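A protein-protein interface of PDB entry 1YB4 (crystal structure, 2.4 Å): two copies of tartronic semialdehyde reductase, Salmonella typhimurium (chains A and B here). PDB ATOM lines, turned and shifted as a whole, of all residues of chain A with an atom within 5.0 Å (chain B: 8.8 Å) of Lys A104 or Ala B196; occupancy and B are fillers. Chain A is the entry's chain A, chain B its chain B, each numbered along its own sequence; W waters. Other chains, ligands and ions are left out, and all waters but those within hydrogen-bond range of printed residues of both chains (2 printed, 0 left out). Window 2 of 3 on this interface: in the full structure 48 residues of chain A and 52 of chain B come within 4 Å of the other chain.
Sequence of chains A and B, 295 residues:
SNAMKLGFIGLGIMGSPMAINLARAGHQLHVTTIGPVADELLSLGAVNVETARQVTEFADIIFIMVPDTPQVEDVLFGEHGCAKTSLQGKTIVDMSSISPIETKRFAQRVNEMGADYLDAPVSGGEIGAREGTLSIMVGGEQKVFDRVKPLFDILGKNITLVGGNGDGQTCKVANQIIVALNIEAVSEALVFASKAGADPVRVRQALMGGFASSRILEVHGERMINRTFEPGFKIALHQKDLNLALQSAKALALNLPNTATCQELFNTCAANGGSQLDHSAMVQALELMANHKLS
Ala B198 touches Asp A167 (CA to OD1, 3.6 Å).
Phe B192 touches Thr A170.
Thr A170 touches Ala B193.
OG1 of Thr A170 touches CB of Ala B196 (3.6 Å).
Ala B198 touches Thr A170 (CB to CG2, 3.7 Å).
The backbone carbonyl oxygen of Gly A166 lies within hydrogen-bond range of the side-chain hydroxyl of Thr A170, 3.0 Å away.
O of Ala B193 sits at hydrogen-bond distance from N of Ala B198 (3.0 Å).
No position is printed for both chains.
Of the 7 pairs that touch across the chains among the printed residues, none has its exchanged pair printed and touching as well.
Hydrophobic or aromatic side chains of chain B that line the printed part of chain A: Phe B192, Ala B193, Ala B196 and Ala B198.
Of the 14 printed residues of chain A, 4 touch a printed residue of chain B.
Among the printed residues, 7 pairs touch across the chains.
Among the printed residues, no Asp or Glu carboxylate lies within 4 Å of a Lys or Arg side-chain nitrogen of the other chain.
Lys A104 touches one residue of chain B.
Of chain A, only Lys A104 (3.0 Å) and Thr A170 (3.6 Å) come within 4 Å of Ala B196.
Of the printed residues of chain A, Phe B192 touches Thr A170 (3.7 Å).
Of the printed residues of chain A, Lys B195 touches Leu A252 (2.8 Å).
The nearest residue of chain B that does not touch Lys A104 is Gly B197 (4.8 Å).
Water W1 lies within hydrogen-bond range of the side-chain carboxylate of Asp A167 (2.4 Å) and the backbone NH of Asp B199 (2.8 Å).
Water W2 lies within hydrogen-bond range of O of Gly B197 (2.5 Å) and OD2 of Asp A167 (2.8 Å).
O of Ala B196 is in hydrogen-bond range of NZ of Lys A104 (3.0 Å).
The backbone carbonyl oxygen of Leu A252 lies within hydrogen-bond range of the side-chain amino group of Lys B195 (2.8 Å).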
ATOM      1  N   PRO A 100     -13.467 -17.531 -25.620  1.00  0.00           N
ATOM      2  CA  PRO A 100     -14.136 -18.578 -26.398  1.00  0.00           C
ATOM      3  C   PRO A 100     -15.662 -18.531 -26.251  1.00  0.00           C
ATOM      4  O   PRO A 100     -16.382 -18.578 -27.245  1.00  0.00           O
ATOM      5  CB  PRO A 100     -13.529 -19.863 -25.835  1.00  0.00           C
ATOM      6  CG  PRO A 100     -12.124 -19.419 -25.468  1.00  0.00           C
ATOM      7  CD  PRO A 100     -12.389 -18.106 -24.789  1.00  0.00           C
ATOM      8  N   ILE A 101     -16.137 -18.425 -25.008  1.00  0.00           N
ATOM      9  CA  ILE A 101     -17.573 -18.351 -24.718  1.00  0.00           C
ATOM     10  C   ILE A 101     -18.206 -17.098 -25.356  1.00  0.00           C
ATOM     11  O   ILE A 101     -19.323 -17.151 -25.891  1.00  0.00           O
ATOM     12  CB  ILE A 101     -17.849 -18.304 -23.182  1.00  0.00           C
ATOM     13  CG1 ILE A 101     -17.319 -19.568 -22.498  1.00  0.00           C
ATOM     14  CG2 ILE A 101     -19.334 -18.171 -22.923  1.00  0.00           C
ATOM     15  CD1 ILE A 101     -15.809 -19.665 -22.461  1.00  0.00           C
ATOM     16  N   GLU A 102     -17.490 -15.976 -25.284  1.00  0.00           N
ATOM     17  CA  GLU A 102     -17.950 -14.712 -25.853  1.00  0.00           C
ATOM     18  C   GLU A 102     -18.079 -14.830 -27.361  1.00  0.00           C
ATOM     19  O   GLU A 102     -19.096 -14.471 -27.942  1.00  0.00           O
ATOM     20  CB  GLU A 102     -16.946 -13.601 -25.547  1.00  0.00           C
ATOM     21  CG  GLU A 102     -16.754 -13.352 -24.092  1.00  0.00           C
ATOM     22  CD  GLU A 102     -18.006 -12.831 -23.468  1.00  0.00           C
ATOM     23  OE1 GLU A 102     -18.332 -11.648 -23.709  1.00  0.00           O
ATOM     24  OE2 GLU A 102     -18.669 -13.613 -22.754  1.00  0.00           O
ATOM     25  N   THR A 103     -17.015 -15.313 -27.989  1.00  0.00           N
ATOM     26  CA  THR A 103     -17.004 -15.481 -29.432  1.00  0.00           C
ATOM     27  C   THR A 103     -18.239 -16.253 -29.880  1.00  0.00           C
ATOM     28  O   THR A 103     -18.830 -15.936 -30.911  1.00  0.00           O
ATOM     29  CB  THR A 103     -15.729 -16.207 -29.889  1.00  0.00           C
ATOM     30  OG1 THR A 103     -14.600 -15.338 -29.704  1.00  0.00           O
ATOM     31  CG2 THR A 103     -15.831 -16.606 -31.354  1.00  0.00           C
ATOM     32  N   LYS A 104     -18.633 -17.255 -29.098  1.00  0.00           N
ATOM     33  CA  LYS A 104     -19.807 -18.048 -29.422  1.00  0.00           C
ATOM     34  C   LYS A 104     -21.000 -17.134 -29.652  1.00  0.00           C
ATOM     35  O   LYS A 104     -21.705 -17.276 -30.649  1.00  0.00           O
ATOM     36  CB  LYS A 104     -20.132 -19.022 -28.286  1.00  0.00           C
ATOM     37  CG  LYS A 104     -19.120 -20.154 -28.075  1.00  0.00           C
ATOM     38  CD  LYS A 104     -19.393 -21.356 -28.978  1.00  0.00           C
ATOM     39  CE  LYS A 104     -18.465 -22.529 -28.651  1.00  0.00           C
ATOM     40  NZ  LYS A 104     -18.682 -23.088 -27.285  1.00  0.00           N
ATOM     41  N   ARG A 105     -21.224 -16.182 -28.750  1.00  0.00           N
ATOM     42  CA  ARG A 105     -22.372 -15.303 -28.924  1.00  0.00           C
ATOM     43  C   ARG A 105     -22.170 -14.133 -29.887  1.00  0.00           C
ATOM     44  O   ARG A 105     -23.130 -13.652 -30.481  1.00  0.00           O
ATOM     45  CB  ARG A 105     -22.903 -14.809 -27.574  1.00  0.00           C
ATOM     46  CG  ARG A 105     -22.092 -13.742 -26.892  1.00  0.00           C
ATOM     47  CD  ARG A 105     -22.949 -13.056 -25.826  1.00  0.00           C
ATOM     48  NE  ARG A 105     -22.198 -12.084 -25.039  1.00  0.00           N
ATOM     49  CZ  ARG A 105     -21.246 -12.401 -24.164  1.00  0.00           C
ATOM     50  NH1 ARG A 105     -20.921 -13.675 -23.957  1.00  0.00           N
ATOM     51  NH2 ARG A 105     -20.623 -11.439 -23.495  1.00  0.00           N
ATOM     52  N   PHE A 106     -20.940 -13.667 -30.055  1.00  0.00           N
ATOM     53  CA  PHE A 106     -20.705 -12.582 -31.006  1.00  0.00           C
ATOM     54  C   PHE A 106     -21.065 -13.140 -32.384  1.00  0.00           C
ATOM     55  O   PHE A 106     -21.754 -12.497 -33.184  1.00  0.00           O
ATOM     56  CB  PHE A 106     -19.232 -12.162 -31.007  1.00  0.00           C
ATOM     57  CG  PHE A 106     -18.793 -11.451 -29.756  1.00  0.00           C
ATOM     58  CD1 PHE A 106     -19.666 -11.277 -28.684  1.00  0.00           C
ATOM     59  CD2 PHE A 106     -17.496 -10.948 -29.653  1.00  0.00           C
ATOM     60  CE1 PHE A 106     -19.251 -10.612 -27.527  1.00  0.00           C
ATOM     61  CE2 PHE A 106     -17.070 -10.282 -28.501  1.00  0.00           C
ATOM     62  CZ  PHE A 106     -17.951 -10.113 -27.433  1.00  0.00           C
ATOM     63  N   ALA A 107     -20.595 -14.361 -32.632  1.00  0.00           N
ATOM     64  CA  ALA A 107     -20.821 -15.060 -33.887  1.00  0.00           C
ATOM     65  C   ALA A 107     -22.295 -15.164 -34.238  1.00  0.00           C
ATOM     66  O   ALA A 107     -22.721 -14.639 -35.265  1.00  0.00           O
ATOM     67  CB  ALA A 107     -20.199 -16.459 -33.832  1.00  0.00           C
ATOM     68  N   GLN A 108     -23.082 -15.831 -33.398  1.00  0.00           N
ATOM     69  CA  GLN A 108     -24.499 -15.977 -33.712  1.00  0.00           C
ATOM     70  C   GLN A 108     -25.220 -14.637 -33.800  1.00  0.00           C
ATOM     71  O   GLN A 108     -26.252 -14.537 -34.458  1.00  0.00           O
ATOM     72  CB  GLN A 108     -25.201 -16.902 -32.715  1.00  0.00           C
ATOM     73  CG  GLN A 108     -25.355 -16.361 -31.320  1.00  0.00           C
ATOM     74  CD  GLN A 108     -26.028 -17.371 -30.403  1.00  0.00           C
ATOM     75  OE1 GLN A 108     -27.107 -17.885 -30.719  1.00  0.00           O
ATOM     76  NE2 GLN A 108     -25.399 -17.661 -29.262  1.00  0.00           N
ATOM     77  N   ASN A 165     -17.565 -22.075 -34.996  1.00  0.00           N
ATOM     78  CA  ASN A 165     -17.337 -20.814 -34.288  1.00  0.00           C
ATOM     79  C   ASN A 165     -17.081 -20.965 -32.797  1.00  0.00           C
ATOM     80  O   ASN A 165     -17.926 -21.471 -32.059  1.00  0.00           O
ATOM     81  CB  ASN A 165     -18.522 -19.871 -34.516  1.00  0.00           C
ATOM     82  CG  ASN A 165     -18.405 -19.096 -35.826  1.00  0.00           C
ATOM     83  OD1 ASN A 165     -19.409 -18.793 -36.472  1.00  0.00           O
ATOM     84  ND2 ASN A 165     -17.172 -18.758 -36.216  1.00  0.00           N
ATOM     85  N   GLY A 166     -15.909 -20.508 -32.364  1.00  0.00           N
ATOM     86  CA  GLY A 166     -15.534 -20.605 -30.966  1.00  0.00           C
ATOM     87  C   GLY A 166     -14.384 -21.578 -30.771  1.00  0.00           C
ATOM     88  O   GLY A 166     -13.581 -21.435 -29.847  1.00  0.00           O
ATOM     89  N   ASP A 167     -14.297 -22.571 -31.649  1.00  0.00           N
ATOM     90  CA  ASP A 167     -13.235 -23.570 -31.562  1.00  0.00           C
ATOM     91  C   ASP A 167     -11.894 -22.968 -31.934  1.00  0.00           C
ATOM     92  O   ASP A 167     -10.845 -23.512 -31.597  1.00  0.00           O
ATOM     93  CB  ASP A 167     -13.532 -24.755 -32.482  1.00  0.00           C
ATOM     94  CG  ASP A 167     -14.697 -25.598 -31.993  1.00  0.00           C
ATOM     95  OD1 ASP A 167     -15.379 -25.184 -31.023  1.00  0.00           O
ATOM     96  OD2 ASP A 167     -14.936 -26.672 -32.591  1.00  0.00           O
ATOM     97  N   THR A 170     -10.887 -21.431 -28.713  1.00  0.00           N
ATOM     98  CA  THR A 170     -10.611 -22.498 -27.787  1.00  0.00           C
ATOM     99  C   THR A 170      -9.280 -23.156 -28.119  1.00  0.00           C
ATOM    100  O   THR A 170      -8.552 -23.598 -27.214  1.00  0.00           O
ATOM    101  CB  THR A 170     -11.722 -23.540 -27.808  1.00  0.00           C
ATOM    102  OG1 THR A 170     -12.934 -22.950 -27.316  1.00  0.00           O
ATOM    103  CG2 THR A 170     -11.324 -24.755 -26.954  1.00  0.00           C
ATOM    104  N   LEU A 252     -16.491 -22.374 -17.256  1.00  0.00           N
ATOM    105  CA  LEU A 252     -16.822 -23.739 -17.630  1.00  0.00           C
ATOM    106  C   LEU A 252     -16.610 -24.679 -16.445  1.00  0.00           C
ATOM    107  O   LEU A 252     -16.787 -25.887 -16.554  1.00  0.00           O
ATOM    108  CB  LEU A 252     -15.934 -24.172 -18.795  1.00  0.00           C
ATOM    109  CG  LEU A 252     -16.095 -23.315 -20.050  1.00  0.00           C
ATOM    110  CD1 LEU A 252     -14.852 -23.414 -20.921  1.00  0.00           C
ATOM    111  CD2 LEU A 252     -17.376 -23.742 -20.774  1.00  0.00           C
ATOM    112  N   ALA B 189      -5.103 -29.017 -21.082  1.00  0.00           N
ATOM    113  CA  ALA B 189      -5.455 -28.395 -22.351  1.00  0.00           C
ATOM    114  C   ALA B 189      -6.573 -29.095 -23.127  1.00  0.00           C
ATOM    115  O   ALA B 189      -7.421 -28.433 -23.725  1.00  0.00           O
ATOM    116  CB  ALA B 189      -4.216 -28.278 -23.218  1.00  0.00           C
ATOM    117  N   LEU B 190      -6.581 -30.425 -23.131  1.00  0.00           N
ATOM    118  CA  LEU B 190      -7.615 -31.153 -23.855  1.00  0.00           C
ATOM    119  C   LEU B 190      -8.960 -31.209 -23.131  1.00  0.00           C
ATOM    120  O   LEU B 190     -10.004 -31.102 -23.758  1.00  0.00           O
ATOM    121  CB  LEU B 190      -7.131 -32.565 -24.177  1.00  0.00           C
ATOM    122  CG  LEU B 190      -6.412 -32.680 -25.519  1.00  0.00           C
ATOM    123  CD1 LEU B 190      -5.321 -33.731 -25.456  1.00  0.00           C
ATOM    124  CD2 LEU B 190      -7.438 -33.028 -26.588  1.00  0.00           C
ATOM    125  N   VAL B 191      -8.940 -31.370 -21.814  1.00  0.00           N
ATOM    126  CA  VAL B 191     -10.183 -31.427 -21.062  1.00  0.00           C
ATOM    127  C   VAL B 191     -10.891 -30.074 -21.101  1.00  0.00           C
ATOM    128  O   VAL B 191     -12.120 -30.007 -21.093  1.00  0.00           O
ATOM    129  CB  VAL B 191      -9.936 -31.847 -19.602  1.00  0.00           C
ATOM    130  CG1 VAL B 191     -11.244 -31.815 -18.815  1.00  0.00           C
ATOM    131  CG2 VAL B 191      -9.349 -33.242 -19.574  1.00  0.00           C
ATOM    132  N   PHE B 192     -10.110 -29.000 -21.153  1.00  0.00           N
ATOM    133  CA  PHE B 192     -10.661 -27.649 -21.216  1.00  0.00           C
ATOM    134  C   PHE B 192     -11.267 -27.457 -22.588  1.00  0.00           C
ATOM    135  O   PHE B 192     -12.367 -26.915 -22.720  1.00  0.00           O
ATOM    136  CB  PHE B 192      -9.554 -26.609 -21.036  1.00  0.00           C
ATOM    137  CG  PHE B 192      -9.828 -25.298 -21.738  1.00  0.00           C
ATOM    138  CD1 PHE B 192     -10.642 -24.338 -21.166  1.00  0.00           C
ATOM    139  CD2 PHE B 192      -9.279 -25.041 -22.990  1.00  0.00           C
ATOM    140  CE1 PHE B 192     -10.905 -23.135 -21.835  1.00  0.00           C
ATOM    141  CE2 PHE B 192      -9.540 -23.843 -23.660  1.00  0.00           C
ATOM    142  CZ  PHE B 192     -10.353 -22.893 -23.080  1.00  0.00           C
ATOM    143  N   ALA B 193     -10.512 -27.874 -23.607  1.00  0.00           N
ATOM    144  CA  ALA B 193     -10.941 -27.749 -24.992  1.00  0.00           C
ATOM    145  C   ALA B 193     -12.234 -28.518 -25.190  1.00  0.00           C
ATOM    146  O   ALA B 193     -13.171 -28.028 -25.815  1.00  0.00           O
ATOM    147  CB  ALA B 193      -9.865 -28.290 -25.933  1.00  0.00           C
ATOM    148  N   SER B 194     -12.280 -29.725 -24.641  1.00  0.00           N
ATOM    149  CA  SER B 194     -13.453 -30.569 -24.764  1.00  0.00           C
ATOM    150  C   SER B 194     -14.696 -29.965 -24.108  1.00  0.00           C
ATOM    151  O   SER B 194     -15.777 -29.945 -24.712  1.00  0.00           O
ATOM    152  CB  SER B 194     -13.163 -31.929 -24.158  1.00  0.00           C
ATOM    153  OG  SER B 194     -14.298 -32.755 -24.246  1.00  0.00           O
ATOM    154  N   LYS B 195     -14.556 -29.482 -22.876  1.00  0.00           N
ATOM    155  CA  LYS B 195     -15.696 -28.887 -22.185  1.00  0.00           C
ATOM    156  C   LYS B 195     -16.036 -27.512 -22.787  1.00  0.00           C
ATOM    157  O   LYS B 195     -17.100 -26.945 -22.512  1.00  0.00           O
ATOM    158  CB  LYS B 195     -15.409 -28.765 -20.681  1.00  0.00           C
ATOM    159  CG  LYS B 195     -16.646 -28.532 -19.843  1.00  0.00           C
ATOM    160  CD  LYS B 195     -16.370 -28.740 -18.370  1.00  0.00           C
ATOM    161  CE  LYS B 195     -17.624 -28.577 -17.527  1.00  0.00           C
ATOM    162  NZ  LYS B 195     -17.299 -28.589 -16.065  1.00  0.00           N
ATOM    163  N   ALA B 196     -15.129 -26.977 -23.602  1.00  0.00           N
ATOM    164  CA  ALA B 196     -15.360 -25.693 -24.251  1.00  0.00           C
ATOM    165  C   ALA B 196     -16.194 -25.958 -25.500  1.00  0.00           C
ATOM    166  O   ALA B 196     -16.776 -25.043 -26.082  1.00  0.00           O
ATOM    167  CB  ALA B 196     -14.032 -25.031 -24.623  1.00  0.00           C
ATOM    168  N   GLY B 197     -16.240 -27.223 -25.909  1.00  0.00           N
ATOM    169  CA  GLY B 197     -17.026 -27.608 -27.073  1.00  0.00           C
ATOM    170  C   GLY B 197     -16.232 -28.028 -28.300  1.00  0.00           C
ATOM    171  O   GLY B 197     -16.794 -28.551 -29.265  1.00  0.00           O
ATOM    172  N   ALA B 198     -14.925 -27.782 -28.256  1.00  0.00           N
ATOM    173  CA  ALA B 198     -14.012 -28.117 -29.348  1.00  0.00           C
ATOM    174  C   ALA B 198     -13.768 -29.631 -29.445  1.00  0.00           C
ATOM    175  O   ALA B 198     -14.018 -30.374 -28.498  1.00  0.00           O
ATOM    176  CB  ALA B 198     -12.694 -27.386 -29.142  1.00  0.00           C
ATOM    177  N   ASP B 199     -13.280 -30.089 -30.592  1.00  0.00           N
ATOM    178  CA  ASP B 199     -13.008 -31.508 -30.772  1.00  0.00           C
ATOM    179  C   ASP B 199     -11.543 -31.851 -30.504  1.00  0.00           C
ATOM    180  O   ASP B 199     -10.643 -31.444 -31.241  1.00  0.00           O
ATOM    181  CB  ASP B 199     -13.428 -31.943 -32.183  1.00  0.00           C
ATOM    182  CG  ASP B 199     -12.758 -33.233 -32.635  1.00  0.00           C
ATOM    183  OD1 ASP B 199     -12.523 -34.131 -31.789  1.00  0.00           O
ATOM    184  OD2 ASP B 199     -12.479 -33.340 -33.854  1.00  0.00           O
ATOM    185  N   PRO B 200     -11.289 -32.602 -29.423  1.00  0.00           N
ATOM    186  CA  PRO B 200      -9.955 -33.032 -29.005  1.00  0.00           C
ATOM    187  C   PRO B 200      -9.086 -33.498 -30.166  1.00  0.00           C
ATOM    188  O   PRO B 200      -7.884 -33.231 -30.205  1.00  0.00           O
ATOM    189  CB  PRO B 200     -10.259 -34.156 -28.024  1.00  0.00           C
ATOM    190  CG  PRO B 200     -11.460 -33.638 -27.333  1.00  0.00           C
ATOM    191  CD  PRO B 200     -12.306 -33.094 -28.476  1.00  0.00           C
ATOM    192  N   VAL B 203      -7.932 -30.167 -32.166  1.00  0.00           N
ATOM    193  CA  VAL B 203      -7.043 -29.361 -31.344  1.00  0.00           C
ATOM    194  C   VAL B 203      -5.655 -30.011 -31.282  1.00  0.00           C
ATOM    195  O   VAL B 203      -4.641 -29.351 -31.538  1.00  0.00           O
ATOM    196  CB  VAL B 203      -7.609 -29.187 -29.914  1.00  0.00           C
ATOM    197  CG1 VAL B 203      -6.756 -28.189 -29.137  1.00  0.00           C
ATOM    198  CG2 VAL B 203      -9.056 -28.705 -29.976  1.00  0.00           C
ATOM    199  N   HIS B 292     -16.247 -34.063 -16.503  1.00  0.00           N
ATOM    200  CA  HIS B 292     -16.398 -34.023 -17.931  1.00  0.00           C
ATOM    201  C   HIS B 292     -15.306 -34.840 -18.625  1.00  0.00           C
ATOM    202  O   HIS B 292     -14.137 -34.454 -18.628  1.00  0.00           O
ATOM    203  CB  HIS B 292     -16.367 -32.565 -18.369  1.00  0.00           C
ATOM    204  CG  HIS B 292     -16.512 -32.376 -19.834  1.00  0.00           C
ATOM    205  ND1 HIS B 292     -15.487 -32.627 -20.720  1.00  0.00           N
ATOM    206  CD2 HIS B 292     -17.564 -31.967 -20.578  1.00  0.00           C
ATOM    207  CE1 HIS B 292     -15.901 -32.379 -21.949  1.00  0.00           C
ATOM    208  NE2 HIS B 292     -17.157 -31.977 -21.890  1.00  0.00           N
ATOM    209  N   LEU B 294     -13.568 -36.765 -22.023  1.00  0.00           N
ATOM    210  CA  LEU B 294     -13.384 -36.400 -23.424  1.00  0.00           C
ATOM    211  C   LEU B 294     -14.356 -37.128 -24.356  1.00  0.00           C
ATOM    212  O   LEU B 294     -15.133 -37.971 -23.869  1.00  0.00           O
ATOM    213  CB  LEU B 294     -11.958 -36.692 -23.871  1.00  0.00           C
ATOM    214  CG  LEU B 294     -10.836 -35.773 -23.394  1.00  0.00           C
ATOM    215  CD1 LEU B 294      -9.514 -36.238 -23.986  1.00  0.00           C
ATOM    216  CD2 LEU B 294     -11.125 -34.365 -23.832  1.00  0.00           C
HETATM  217  O   HOH W   1     -13.443 -28.556 -32.976  1.00  0.00           O
HETATM  218  O   HOH W   2     -17.302 -27.823 -31.654  1.00  0.00           O
